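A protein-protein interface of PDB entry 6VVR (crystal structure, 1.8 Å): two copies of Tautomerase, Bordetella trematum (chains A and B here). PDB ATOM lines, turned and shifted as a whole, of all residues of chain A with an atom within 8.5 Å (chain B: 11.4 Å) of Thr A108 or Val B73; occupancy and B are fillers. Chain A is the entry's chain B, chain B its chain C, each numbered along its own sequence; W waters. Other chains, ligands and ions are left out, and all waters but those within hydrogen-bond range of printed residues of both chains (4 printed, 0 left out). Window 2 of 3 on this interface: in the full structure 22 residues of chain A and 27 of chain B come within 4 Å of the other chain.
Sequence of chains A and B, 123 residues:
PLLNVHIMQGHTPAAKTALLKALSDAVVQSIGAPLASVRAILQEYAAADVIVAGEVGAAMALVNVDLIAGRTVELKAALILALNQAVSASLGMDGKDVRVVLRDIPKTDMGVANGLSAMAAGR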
ATOM      1  N   ILE A  68     -23.394  18.216   7.486  1.00  0.00           N
ATOM      2  CA  ILE A  68     -24.572  17.444   7.858  1.00  0.00           C
ATOM      3  C   ILE A  68     -25.193  16.811   6.624  1.00  0.00           C
ATOM      4  O   ILE A  68     -25.325  17.445   5.568  1.00  0.00           O
ATOM      5  CB  ILE A  68     -25.569  18.334   8.611  1.00  0.00           C
ATOM      6  CG1 ILE A  68     -24.943  18.774   9.944  1.00  0.00           C
ATOM      7  CG2 ILE A  68     -26.876  17.589   8.825  1.00  0.00           C
ATOM      8  CD1 ILE A  68     -25.821  19.720  10.754  1.00  0.00           C
ATOM      9  N   ALA A  69     -25.581  15.546   6.756  1.00  0.00           N
ATOM     10  CA  ALA A  69     -26.133  14.805   5.641  1.00  0.00           C
ATOM     11  C   ALA A  69     -27.443  15.434   5.174  1.00  0.00           C
ATOM     12  O   ALA A  69     -28.123  16.149   5.919  1.00  0.00           O
ATOM     13  CB  ALA A  69     -26.353  13.348   6.047  1.00  0.00           C
ATOM     14  N   ILE A 105     -22.325  13.752   7.408  1.00  0.00           N
ATOM     15  CA  ILE A 105     -22.386  13.439   8.833  1.00  0.00           C
ATOM     16  C   ILE A 105     -23.859  13.476   9.250  1.00  0.00           C
ATOM     17  O   ILE A 105     -24.483  14.536   9.169  1.00  0.00           O
ATOM     18  CB  ILE A 105     -21.562  14.439   9.662  1.00  0.00           C
ATOM     19  CG1 ILE A 105     -20.139  14.581   9.100  1.00  0.00           C
ATOM     20  CG2 ILE A 105     -21.542  14.036  11.145  1.00  0.00           C
ATOM     21  CD1 ILE A 105     -19.347  13.271   9.033  1.00  0.00           C
ATOM     22  N   PRO A 106     -24.438  12.363   9.696  1.00  0.00           N
ATOM     23  CA  PRO A 106     -25.802  12.427  10.243  1.00  0.00           C
ATOM     24  C   PRO A 106     -25.898  13.430  11.386  1.00  0.00           C
ATOM     25  O   PRO A 106     -24.932  13.680  12.113  1.00  0.00           O
ATOM     26  CB  PRO A 106     -26.057  10.990  10.721  1.00  0.00           C
ATOM     27  CG  PRO A 106     -25.166  10.136   9.836  1.00  0.00           C
ATOM     28  CD  PRO A 106     -23.919  10.988   9.635  1.00  0.00           C
ATOM     29  N   LYS A 107     -27.098  14.001  11.542  1.00  0.00           N
ATOM     30  CA  LYS A 107     -27.317  15.027  12.565  1.00  0.00           C
ATOM     31  C   LYS A 107     -27.018  14.496  13.964  1.00  0.00           C
ATOM     32  O   LYS A 107     -26.588  15.244  14.854  1.00  0.00           O
ATOM     33  CB  LYS A 107     -28.754  15.548  12.523  1.00  0.00           C
ATOM     34  CG  LYS A 107     -29.165  16.385  11.336  1.00  0.00           C
ATOM     35  CD  LYS A 107     -29.326  15.385  10.143  1.00  0.00           C
ATOM     36  CE  LYS A 107     -30.179  14.254  10.555  1.00  0.00           C
ATOM     37  NZ  LYS A 107     -29.812  13.192   9.582  1.00  0.00           N
ATOM     38  N   THR A 108     -27.232  13.195  14.171  1.00  0.00           N
ATOM     39  CA  THR A 108     -26.937  12.582  15.460  1.00  0.00           C
ATOM     40  C   THR A 108     -25.444  12.554  15.718  1.00  0.00           C
ATOM     41  O   THR A 108     -25.017  12.436  16.873  1.00  0.00           O
ATOM     42  CB  THR A 108     -27.485  11.154  15.511  1.00  0.00           C
ATOM     43  OG1 THR A 108     -26.909  10.396  14.442  1.00  0.00           O
ATOM     44  CG2 THR A 108     -29.009  11.147  15.380  1.00  0.00           C
ATOM     45  N   ASP A 109     -24.639  12.658  14.654  1.00  0.00           N
ATOM     46  CA  ASP A 109     -23.195  12.498  14.739  1.00  0.00           C
ATOM     47  C   ASP A 109     -22.441  13.816  14.686  1.00  0.00           C
ATOM     48  O   ASP A 109     -21.226  13.820  14.909  1.00  0.00           O
ATOM     49  CB  ASP A 109     -22.671  11.613  13.601  1.00  0.00           C
ATOM     50  CG  ASP A 109     -23.270  10.220  13.607  1.00  0.00           C
ATOM     51  OD1 ASP A 109     -24.056   9.901  14.526  1.00  0.00           O
ATOM     52  OD2 ASP A 109     -22.939   9.438  12.685  1.00  0.00           O
ATOM     53  N   MET A 110     -23.126  14.916  14.382  1.00  0.00           N
ATOM     54  CA  MET A 110     -22.505  16.225  14.240  1.00  0.00           C
ATOM     55  C   MET A 110     -22.725  17.028  15.513  1.00  0.00           C
ATOM     56  O   MET A 110     -23.865  17.356  15.852  1.00  0.00           O
ATOM     57  CB  MET A 110     -23.085  16.970  13.037  1.00  0.00           C
ATOM     58  CG  MET A 110     -22.550  18.387  12.901  1.00  0.00           C
ATOM     59  SD  MET A 110     -20.818  18.382  12.378  1.00  0.00           S
ATOM     60  CE  MET A 110     -21.011  17.861  10.684  1.00  0.00           C
ATOM     61  N   GLY A 111     -21.638  17.346  16.209  1.00  0.00           N
ATOM     62  CA  GLY A 111     -21.738  18.205  17.365  1.00  0.00           C
ATOM     63  C   GLY A 111     -21.888  19.660  16.952  1.00  0.00           C
ATOM     64  O   GLY A 111     -21.318  20.116  15.957  1.00  0.00           O
ATOM     65  N   VAL A 112     -22.680  20.389  17.725  1.00  0.00           N
ATOM     66  CA  VAL A 112     -22.778  21.829  17.528  1.00  0.00           C
ATOM     67  C   VAL A 112     -22.300  22.497  18.813  1.00  0.00           C
ATOM     68  O   VAL A 112     -21.563  21.890  19.603  1.00  0.00           O
ATOM     69  CB  VAL A 112     -24.209  22.251  17.131  1.00  0.00           C
ATOM     70  CG1 VAL A 112     -24.556  21.702  15.740  1.00  0.00           C
ATOM     71  CG2 VAL A 112     -25.221  21.767  18.154  1.00  0.00           C
ATOM     72  N   LEU A 116     -23.796  19.579  22.143  1.00  0.00           N
ATOM     73  CA  LEU A 116     -25.029  18.942  21.710  1.00  0.00           C
ATOM     74  C   LEU A 116     -24.888  18.472  20.269  1.00  0.00           C
ATOM     75  O   LEU A 116     -24.163  19.076  19.476  1.00  0.00           O
ATOM     76  CB  LEU A 116     -26.213  19.901  21.824  1.00  0.00           C
ATOM     77  CG  LEU A 116     -26.568  20.300  23.252  1.00  0.00           C
ATOM     78  CD1 LEU A 116     -27.461  21.539  23.264  1.00  0.00           C
ATOM     79  CD2 LEU A 116     -27.239  19.125  23.939  1.00  0.00           C
ATOM     80  N   SER A 117     -25.584  17.388  19.930  1.00  0.00           N
ATOM     81  CA  SER A 117     -25.644  17.019  18.524  1.00  0.00           C
ATOM     82  C   SER A 117     -26.525  18.007  17.766  1.00  0.00           C
ATOM     83  O   SER A 117     -27.344  18.726  18.345  1.00  0.00           O
ATOM     84  CB  SER A 117     -26.185  15.604  18.334  1.00  0.00           C
ATOM     85  OG  SER A 117     -27.594  15.569  18.518  1.00  0.00           O
ATOM     86  N   ALA A 118     -26.342  18.037  16.447  1.00  0.00           N
ATOM     87  CA  ALA A 118     -27.195  18.874  15.619  1.00  0.00           C
ATOM     88  C   ALA A 118     -28.654  18.459  15.728  1.00  0.00           C
ATOM     89  O   ALA A 118     -29.542  19.289  15.529  1.00  0.00           O
ATOM     90  CB  ALA A 118     -26.730  18.819  14.166  1.00  0.00           C
ATOM     91  N   MET A 119     -28.917  17.196  16.055  1.00  0.00           N
ATOM     92  CA  MET A 119     -30.290  16.749  16.254  1.00  0.00           C
ATOM     93  C   MET A 119     -30.859  17.263  17.573  1.00  0.00           C
ATOM     94  O   MET A 119     -32.022  17.680  17.628  1.00  0.00           O
ATOM     95  CB  MET A 119     -30.350  15.222  16.198  1.00  0.00           C
ATOM     96  CG  MET A 119     -31.728  14.671  15.882  1.00  0.00           C
ATOM     97  SD  MET A 119     -31.917  13.003  16.538  1.00  0.00           S
ATOM     98  CE  MET A 119     -31.293  13.230  18.205  1.00  0.00           C
ATOM     99  N   ALA A 120     -30.059  17.245  18.643  1.00  0.00           N
ATOM    100  CA  ALA A 120     -30.526  17.766  19.925  1.00  0.00           C
ATOM    101  C   ALA A 120     -30.843  19.253  19.843  1.00  0.00           C
ATOM    102  O   ALA A 120     -31.660  19.757  20.622  1.00  0.00           O
ATOM    103  CB  ALA A 120     -29.484  17.502  21.012  1.00  0.00           C
ATOM    104  N   SER B  30     -17.720   7.779  28.608  1.00  0.00           N
ATOM    105  CA  SER B  30     -19.010   8.082  28.003  1.00  0.00           C
ATOM    106  C   SER B  30     -19.566   6.938  27.158  1.00  0.00           C
ATOM    107  O   SER B  30     -20.788   6.774  27.090  1.00  0.00           O
ATOM    108  CB  SER B  30     -18.915   9.353  27.144  1.00  0.00           C
ATOM    109  OG  SER B  30     -18.072   9.145  26.032  1.00  0.00           O
ATOM    110  N   ILE B  31     -18.721   6.148  26.497  1.00  0.00           N
ATOM    111  CA  ILE B  31     -19.195   5.037  25.673  1.00  0.00           C
ATOM    112  C   ILE B  31     -18.581   3.699  26.074  1.00  0.00           C
ATOM    113  O   ILE B  31     -18.870   2.689  25.421  1.00  0.00           O
ATOM    114  CB  ILE B  31     -18.982   5.296  24.170  1.00  0.00           C
ATOM    115  CG1 ILE B  31     -17.497   5.233  23.800  1.00  0.00           C
ATOM    116  CG2 ILE B  31     -19.600   6.638  23.754  1.00  0.00           C
ATOM    117  CD1 ILE B  31     -17.253   5.299  22.306  1.00  0.00           C
ATOM    118  N   VAL B  63     -12.727  18.550  17.514  1.00  0.00           N
ATOM    119  CA  VAL B  63     -12.401  17.171  17.849  1.00  0.00           C
ATOM    120  C   VAL B  63     -13.055  16.289  16.804  1.00  0.00           C
ATOM    121  O   VAL B  63     -14.285  16.156  16.782  1.00  0.00           O
ATOM    122  CB  VAL B  63     -12.882  16.777  19.250  1.00  0.00           C
ATOM    123  CG1 VAL B  63     -12.445  15.350  19.552  1.00  0.00           C
ATOM    124  CG2 VAL B  63     -12.338  17.744  20.291  1.00  0.00           C
ATOM    125  N   VAL B  65     -13.586  12.493  15.467  1.00  0.00           N
ATOM    126  CA  VAL B  65     -13.593  11.158  16.051  1.00  0.00           C
ATOM    127  C   VAL B  65     -13.937  10.153  14.958  1.00  0.00           C
ATOM    128  O   VAL B  65     -15.057  10.165  14.431  1.00  0.00           O
ATOM    129  CB  VAL B  65     -14.612  11.032  17.191  1.00  0.00           C
ATOM    130  CG1 VAL B  65     -14.471   9.672  17.850  1.00  0.00           C
ATOM    131  CG2 VAL B  65     -14.492  12.172  18.191  1.00  0.00           C
ATOM    132  N   LEU B  67     -14.732   6.390  14.769  1.00  0.00           N
ATOM    133  CA  LEU B  67     -15.065   5.321  15.706  1.00  0.00           C
ATOM    134  C   LEU B  67     -15.901   4.255  15.008  1.00  0.00           C
ATOM    135  O   LEU B  67     -16.622   4.524  14.043  1.00  0.00           O
ATOM    136  CB  LEU B  67     -15.797   5.856  16.958  1.00  0.00           C
ATOM    137  CG  LEU B  67     -17.313   6.153  16.901  1.00  0.00           C
ATOM    138  CD1 LEU B  67     -17.897   6.419  18.285  1.00  0.00           C
ATOM    139  CD2 LEU B  67     -17.610   7.324  16.003  1.00  0.00           C
ATOM    140  N   ILE B  68     -15.784   3.023  15.511  1.00  0.00           N
ATOM    141  CA  ILE B  68     -16.517   1.899  14.937  1.00  0.00           C
ATOM    142  C   ILE B  68     -18.013   2.161  14.996  1.00  0.00           C
ATOM    143  O   ILE B  68     -18.545   2.611  16.018  1.00  0.00           O
ATOM    144  CB  ILE B  68     -16.139   0.601  15.665  1.00  0.00           C
ATOM    145  CG1 ILE B  68     -14.714   0.203  15.270  1.00  0.00           C
ATOM    146  CG2 ILE B  68     -17.143  -0.527  15.338  1.00  0.00           C
ATOM    147  CD1 ILE B  68     -14.087  -0.829  16.174  1.00  0.00           C
ATOM    148  N   ALA B  69     -18.697   1.865  13.892  1.00  0.00           N
ATOM    149  CA  ALA B  69     -20.129   2.074  13.770  1.00  0.00           C
ATOM    150  C   ALA B  69     -20.890   1.244  14.794  1.00  0.00           C
ATOM    151  O   ALA B  69     -20.404   0.229  15.295  1.00  0.00           O
ATOM    152  CB  ALA B  69     -20.614   1.695  12.368  1.00  0.00           C
ATOM    153  N   GLY B  70     -22.115   1.675  15.074  1.00  0.00           N
ATOM    154  CA  GLY B  70     -23.018   0.900  15.910  1.00  0.00           C
ATOM    155  C   GLY B  70     -23.350   1.510  17.255  1.00  0.00           C
ATOM    156  O   GLY B  70     -24.242   0.985  17.938  1.00  0.00           O
ATOM    157  N   ARG B  71     -22.677   2.569  17.703  1.00  0.00           N
ATOM    158  CA  ARG B  71     -23.064   3.203  18.959  1.00  0.00           C
ATOM    159  C   ARG B  71     -24.458   3.811  18.833  1.00  0.00           C
ATOM    160  O   ARG B  71     -24.815   4.369  17.793  1.00  0.00           O
ATOM    161  CB  ARG B  71     -22.049   4.280  19.357  1.00  0.00           C
ATOM    162  CG  ARG B  71     -20.902   3.774  20.246  1.00  0.00           C
ATOM    163  CD  ARG B  71     -19.818   3.055  19.453  1.00  0.00           C
ATOM    164  NE  ARG B  71     -18.739   2.578  20.321  1.00  0.00           N
ATOM    165  CZ  ARG B  71     -17.488   2.370  19.918  1.00  0.00           C
ATOM    166  NH1 ARG B  71     -17.147   2.595  18.654  1.00  0.00           N
ATOM    167  NH2 ARG B  71     -16.568   1.941  20.782  1.00  0.00           N
ATOM    168  N   THR B  72     -25.261   3.677  19.889  1.00  0.00           N
ATOM    169  CA  THR B  72     -26.587   4.275  19.874  1.00  0.00           C
ATOM    170  C   THR B  72     -26.492   5.796  19.816  1.00  0.00           C
ATOM    171  O   THR B  72     -25.470   6.393  20.156  1.00  0.00           O
ATOM    172  CB  THR B  72     -27.386   3.865  21.113  1.00  0.00           C
ATOM    173  OG1 THR B  72     -26.763   4.403  22.285  1.00  0.00           O
ATOM    174  CG2 THR B  72     -27.449   2.361  21.233  1.00  0.00           C
ATOM    175  N   VAL B  73     -27.591   6.424  19.381  1.00  0.00           N
ATOM    176  CA  VAL B  73     -27.681   7.887  19.408  1.00  0.00           C
ATOM    177  C   VAL B  73     -27.429   8.410  20.817  1.00  0.00           C
ATOM    178  O   VAL B  73     -26.771   9.443  21.014  1.00  0.00           O
ATOM    179  CB  VAL B  73     -29.056   8.340  18.873  1.00  0.00           C
ATOM    180  CG1 VAL B  73     -29.289   9.836  19.120  1.00  0.00           C
ATOM    181  CG2 VAL B  73     -29.179   8.003  17.384  1.00  0.00           C
ATOM    182  N   GLU B  74     -27.952   7.702  21.819  1.00  0.00           N
ATOM    183  CA  GLU B  74     -27.756   8.089  23.210  1.00  0.00           C
ATOM    184  C   GLU B  74     -26.274   8.078  23.595  1.00  0.00           C
ATOM    185  O   GLU B  74     -25.787   9.014  24.241  1.00  0.00           O
ATOM    186  CB  GLU B  74     -28.577   7.151  24.105  1.00  0.00           C
ATOM    187  CG  GLU B  74     -28.472   7.416  25.583  1.00  0.00           C
ATOM    188  CD  GLU B  74     -29.370   6.499  26.402  1.00  0.00           C
ATOM    189  OE1 GLU B  74     -29.448   5.283  26.095  1.00  0.00           O
ATOM    190  OE2 GLU B  74     -30.008   6.999  27.348  1.00  0.00           O
ATOM    191  N   LEU B  75     -25.535   7.038  23.193  1.00  0.00           N
ATOM    192  CA  LEU B  75     -24.105   7.003  23.502  1.00  0.00           C
ATOM    193  C   LEU B  75     -23.357   8.108  22.772  1.00  0.00           C
ATOM    194  O   LEU B  75     -22.429   8.713  23.326  1.00  0.00           O
ATOM    195  CB  LEU B  75     -23.501   5.644  23.135  1.00  0.00           C
ATOM    196  CG  LEU B  75     -23.700   4.486  24.112  1.00  0.00           C
ATOM    197  CD1 LEU B  75     -22.634   3.407  23.934  1.00  0.00           C
ATOM    198  CD2 LEU B  75     -23.647   5.024  25.472  1.00  0.00           C
ATOM    199  N   LYS B  76     -23.731   8.364  21.518  1.00  0.00           N
ATOM    200  CA  LYS B  76     -23.079   9.421  20.749  1.00  0.00           C
ATOM    201  C   LYS B  76     -23.307  10.781  21.392  1.00  0.00           C
ATOM    202  O   LYS B  76     -22.398  11.610  21.444  1.00  0.00           O
ATOM    203  CB  LYS B  76     -23.599   9.412  19.311  1.00  0.00           C
ATOM    204  CG  LYS B  76     -23.165   8.202  18.499  1.00  0.00           C
ATOM    205  CD  LYS B  76     -23.873   8.163  17.137  1.00  0.00           C
ATOM    206  CE  LYS B  76     -23.235   7.133  16.219  1.00  0.00           C
ATOM    207  NZ  LYS B  76     -23.891   7.034  14.886  1.00  0.00           N
ATOM    208  N   ALA B  77     -24.515  11.024  21.902  1.00  0.00           N
ATOM    209  CA  ALA B  77     -24.780  12.282  22.588  1.00  0.00           C
ATOM    210  C   ALA B  77     -23.911  12.428  23.832  1.00  0.00           C
ATOM    211  O   ALA B  77     -23.364  13.505  24.086  1.00  0.00           O
ATOM    212  CB  ALA B  77     -26.265  12.382  22.942  1.00  0.00           C
ATOM    213  N   ALA B  78     -23.762  11.355  24.614  1.00  0.00           N
ATOM    214  CA  ALA B  78     -22.888  11.409  25.782  1.00  0.00           C
ATOM    215  C   ALA B  78     -21.446  11.653  25.372  1.00  0.00           C
ATOM    216  O   ALA B  78     -20.717  12.403  26.035  1.00  0.00           O
ATOM    217  CB  ALA B  78     -22.994  10.108  26.580  1.00  0.00           C
ATOM    218  N   LEU B  79     -21.017  11.027  24.280  1.00  0.00           N
ATOM    219  CA  LEU B  79     -19.641  11.191  23.827  1.00  0.00           C
ATOM    220  C   LEU B  79     -19.391  12.620  23.364  1.00  0.00           C
ATOM    221  O   LEU B  79     -18.395  13.247  23.749  1.00  0.00           O
ATOM    222  CB  LEU B  79     -19.344  10.191  22.709  1.00  0.00           C
ATOM    223  CG  LEU B  79     -17.981  10.351  22.027  1.00  0.00           C
ATOM    224  CD1 LEU B  79     -16.852  10.158  23.008  1.00  0.00           C
ATOM    225  CD2 LEU B  79     -17.868   9.362  20.866  1.00  0.00           C
ATOM    226  N   ILE B  80     -20.290  13.150  22.539  1.00  0.00           N
ATOM    227  CA  ILE B  80     -20.138  14.516  22.048  1.00  0.00           C
ATOM    228  C   ILE B  80     -20.083  15.493  23.216  1.00  0.00           C
ATOM    229  O   ILE B  80     -19.225  16.385  23.266  1.00  0.00           O
ATOM    230  CB  ILE B  80     -21.283  14.844  21.071  1.00  0.00           C
ATOM    231  CG1 ILE B  80     -21.123  14.022  19.789  1.00  0.00           C
ATOM    232  CG2 ILE B  80     -21.315  16.318  20.742  1.00  0.00           C
ATOM    233  CD1 ILE B  80     -22.325  14.080  18.853  1.00  0.00           C
ATOM    234  N   LEU B  81     -20.982  15.325  24.188  1.00  0.00           N
ATOM    235  CA  LEU B  81     -21.000  16.238  25.326  1.00  0.00           C
ATOM    236  C   LEU B  81     -19.728  16.108  26.154  1.00  0.00           C
ATOM    237  O   LEU B  81     -19.129  17.118  26.539  1.00  0.00           O
ATOM    238  CB  LEU B  81     -22.236  15.982  26.185  1.00  0.00           C
ATOM    239  CG  LEU B  81     -22.404  16.907  27.395  1.00  0.00           C
ATOM    240  CD1 LEU B  81     -22.530  18.351  26.957  1.00  0.00           C
ATOM    241  CD2 LEU B  81     -23.623  16.488  28.201  1.00  0.00           C
ATOM    242  N   ALA B  82     -19.283  14.873  26.405  1.00  0.00           N
ATOM    243  CA  ALA B  82     -18.112  14.656  27.244  1.00  0.00           C
ATOM    244  C   ALA B  82     -16.850  15.212  26.598  1.00  0.00           C
ATOM    245  O   ALA B  82     -15.988  15.758  27.294  1.00  0.00           O
ATOM    246  CB  ALA B  82     -17.942  13.163  27.547  1.00  0.00           C
ATOM    247  N   LEU B  83     -16.722  15.080  25.269  1.00  0.00           N
ATOM    248  CA  LEU B  83     -15.544  15.619  24.593  1.00  0.00           C
ATOM    249  C   LEU B  83     -15.562  17.143  24.592  1.00  0.00           C
ATOM    250  O   LEU B  83     -14.515  17.781  24.769  1.00  0.00           O
ATOM    251  CB  LEU B  83     -15.465  15.098  23.160  1.00  0.00           C
ATOM    252  CG  LEU B  83     -15.259  13.592  23.026  1.00  0.00           C
ATOM    253  CD1 LEU B  83     -15.366  13.190  21.552  1.00  0.00           C
ATOM    254  CD2 LEU B  83     -13.928  13.178  23.615  1.00  0.00           C
ATOM    255  N   VAL B 100     -17.410  19.028  17.775  1.00  0.00           N
ATOM    256  CA  VAL B 100     -17.085  17.607  17.799  1.00  0.00           C
ATOM    257  C   VAL B 100     -17.744  16.969  16.586  1.00  0.00           C
ATOM    258  O   VAL B 100     -18.934  17.189  16.344  1.00  0.00           O
ATOM    259  CB  VAL B 100     -17.595  16.933  19.089  1.00  0.00           C
ATOM    260  CG1 VAL B 100     -17.398  15.434  19.015  1.00  0.00           C
ATOM    261  CG2 VAL B 100     -16.911  17.535  20.314  1.00  0.00           C
ATOM    262  N   VAL B 101     -16.985  16.188  15.824  1.00  0.00           N
ATOM    263  CA  VAL B 101     -17.533  15.468  14.679  1.00  0.00           C
ATOM    264  C   VAL B 101     -17.245  13.988  14.868  1.00  0.00           C
ATOM    265  O   VAL B 101     -16.081  13.591  14.992  1.00  0.00           O
ATOM    266  CB  VAL B 101     -16.943  15.964  13.348  1.00  0.00           C
ATOM    267  CG1 VAL B 101     -17.550  15.178  12.190  1.00  0.00           C
ATOM    268  CG2 VAL B 101     -17.185  17.467  13.184  1.00  0.00           C
ATOM    269  N   LEU B 102     -18.298  13.174  14.862  1.00  0.00           N
ATOM    270  CA  LEU B 102     -18.160  11.723  14.910  1.00  0.00           C
ATOM    271  C   LEU B 102     -18.321  11.158  13.507  1.00  0.00           C
ATOM    272  O   LEU B 102     -19.301  11.465  12.828  1.00  0.00           O
ATOM    273  CB  LEU B 102     -19.211  11.096  15.828  1.00  0.00           C
ATOM    274  CG  LEU B 102     -19.462  11.674  17.215  1.00  0.00           C
ATOM    275  CD1 LEU B 102     -20.569  10.866  17.917  1.00  0.00           C
ATOM    276  CD2 LEU B 102     -18.194  11.673  18.043  1.00  0.00           C
ATOM    277  N   ARG B 103     -17.385  10.307  13.093  1.00  0.00           N
ATOM    278  CA  ARG B 103     -17.461   9.602  11.815  1.00  0.00           C
ATOM    279  C   ARG B 103     -17.612   8.108  12.094  1.00  0.00           C
ATOM    280  O   ARG B 103     -16.670   7.461  12.566  1.00  0.00           O
ATOM    281  CB  ARG B 103     -16.226   9.887  10.960  1.00  0.00           C
ATOM    282  CG  ARG B 103     -15.987  11.376  10.750  1.00  0.00           C
ATOM    283  CD  ARG B 103     -15.088  11.632   9.562  1.00  0.00           C
ATOM    284  NE  ARG B 103     -14.551  12.991   9.562  1.00  0.00           N
ATOM    285  CZ  ARG B 103     -13.363  13.313  10.052  1.00  0.00           C
ATOM    286  NH1 ARG B 103     -12.940  14.572   9.987  1.00  0.00           N
ATOM    287  NH2 ARG B 103     -12.593  12.368  10.588  1.00  0.00           N
ATOM    288  N   ASP B 104     -18.800   7.571  11.813  1.00  0.00           N
ATOM    289  CA  ASP B 104     -19.054   6.142  11.969  1.00  0.00           C
ATOM    290  C   ASP B 104     -18.286   5.368  10.902  1.00  0.00           C
ATOM    291  O   ASP B 104     -18.504   5.566   9.701  1.00  0.00           O
ATOM    292  CB  ASP B 104     -20.549   5.844  11.847  1.00  0.00           C
ATOM    293  CG  ASP B 104     -21.279   5.882  13.184  1.00  0.00           C
ATOM    294  OD1 ASP B 104     -20.638   6.053  14.241  1.00  0.00           O
ATOM    295  OD2 ASP B 104     -22.518   5.756  13.168  1.00  0.00           O
HETATM  296  O   HOH W   1     -20.778   9.711  11.210  1.00  0.00           O
HETATM  297  O   HOH W   2     -19.799  19.974  19.447  1.00  0.00           O
HETATM  298  O   HOH W   3     -23.982   7.214  11.550  1.00  0.00           O
HETATM  299  O   HOH W   4     -26.418  11.854  19.356  1.00  0.00           O
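The backbone NH (N) of Gly A111 lies within hydrogen-bond range of the backbone carbonyl oxygen (O) of Val B100.
The backbone carbonyl oxygen of Asp A109 lies within hydrogen-bond range of the backbone NH of Leu B102, 3.0 Å away.
OD1 of Asp A109 is in salt-bridge range of NZ of Lys B76, at 2.9 Å.
The backbone carbonyl oxygen (O) of Met A110 sits at hydrogen-bond distance from the backbone NH (N) of Ala A118 (2.6 Å).
The side-chain hydroxyl (OG1) of Thr A108 sits at hydrogen-bond distance from the side-chain carboxylate (OD1) of Asp A109, 2.9 Å away.
The backbone carbonyl oxygen (O) of Val B63 sits at hydrogen-bond distance from the backbone NH (N) of Val B101 (2.9 Å).
O of Ile A105 lies within hydrogen-bond range of N of Ala A69.
The side-chain amino group (NZ) of Lys B76 lies within salt-bridge range of the side-chain carboxylate (OD2) of Asp B104.
The backbone NH (N) of Val B65 lies within hydrogen-bond range of the backbone carbonyl oxygen (O) of Val B101, 2.8 Å away.
Ile A105 touches Leu B102.
Val B73 touches Thr A108 (CG2 to CG2, 3.7 Å).
Thr A108 touches Ile B80.
Asp A109 touches Val B101.
Asp A109 touches Asp B104.
Met A110 touches Val B100 (C to O, 3.9 Å).
Val B101 touches Met A110 (CG2 to SD, 3.8 Å).
Gly A111 touches Ile B80 (CA to CG2, 3.9 Å).
Of chain B, only Val B73 (3.7 Å) and Ile B80 (3.7 Å) come within 4 Å of Thr A108.
Val B73 touches one residue of chain A.
No residue of chain B comes within 4 Å of Lys A107.
No residue of chain B comes within 4 Å of Ser A117.
No residue of chain B comes within 4 Å of Ala A118.
Of the printed residues of chain B, Ile A105 touches Leu B102 (3.8 Å).
Printed residues of chain A within 4 Å of Lys B76: Asp A109 (2.9 Å).
Printed residues of chain B within 4 Å of Gly A111: Ile B80 and Val B100.
Of the printed residues of chain A, Asp B104 touches Asp A109.
Leu B67 touches none of the printed residues of chain A.
Ala B78 touches none of the printed residues of chain A.
The nearest residue of chain A that does not touch Val B73 is Met A119 (4.05 Å).
Of the 26 printed residues of chain B, 7 touch a printed residue of chain A.
Printed residues of chain B that touch a printed residue of chain A: Val B73, Lys B76, Ile B80, Val B100, Val B101, Leu B102 and Asp B104.
Of the 15 printed residues of chain A, 5 touch a printed residue of chain B.
Hydrophobic or aromatic side chains of chain A that line the printed part of chain B: Ile A105 and Met A110.
Among the printed residues, 11 pairs touch across the chains.
Among the printed residues, Asp or Glu carboxylates within 4 Å of a Lys or Arg side-chain nitrogen of the other chain: Asp A109 with Lys B76 (2.9 Å).
Positions printed for both chains: 68 and 69.
Of the 11 pairs that touch across the chains among the printed residues, none has its exchanged pair printed and touching as well.
Water W2 lies within hydrogen-bond range of O of Val A112 (2.6 Å) and N of Val B100 (3.1 Å).
Water W3 lies within hydrogen-bond range of the side-chain carboxylate of Asp B104 (2.6 Å), the side-chain carboxylate of Asp A109 (2.7 Å) and the side-chain amino group of Lys B76 (3.3 Å).
Water W1 lies within hydrogen-bond range of OD2 of Asp A109 (2.6 Å), O of Leu B102 (2.8 Å) and N of Asp B104 (3.0 Å).
Water W4 lies within hydrogen-bond range of O of Thr A108 (2.9 Å), O of Val B73 (2.9 Å) and N of Ala B77 (3.3 Å).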
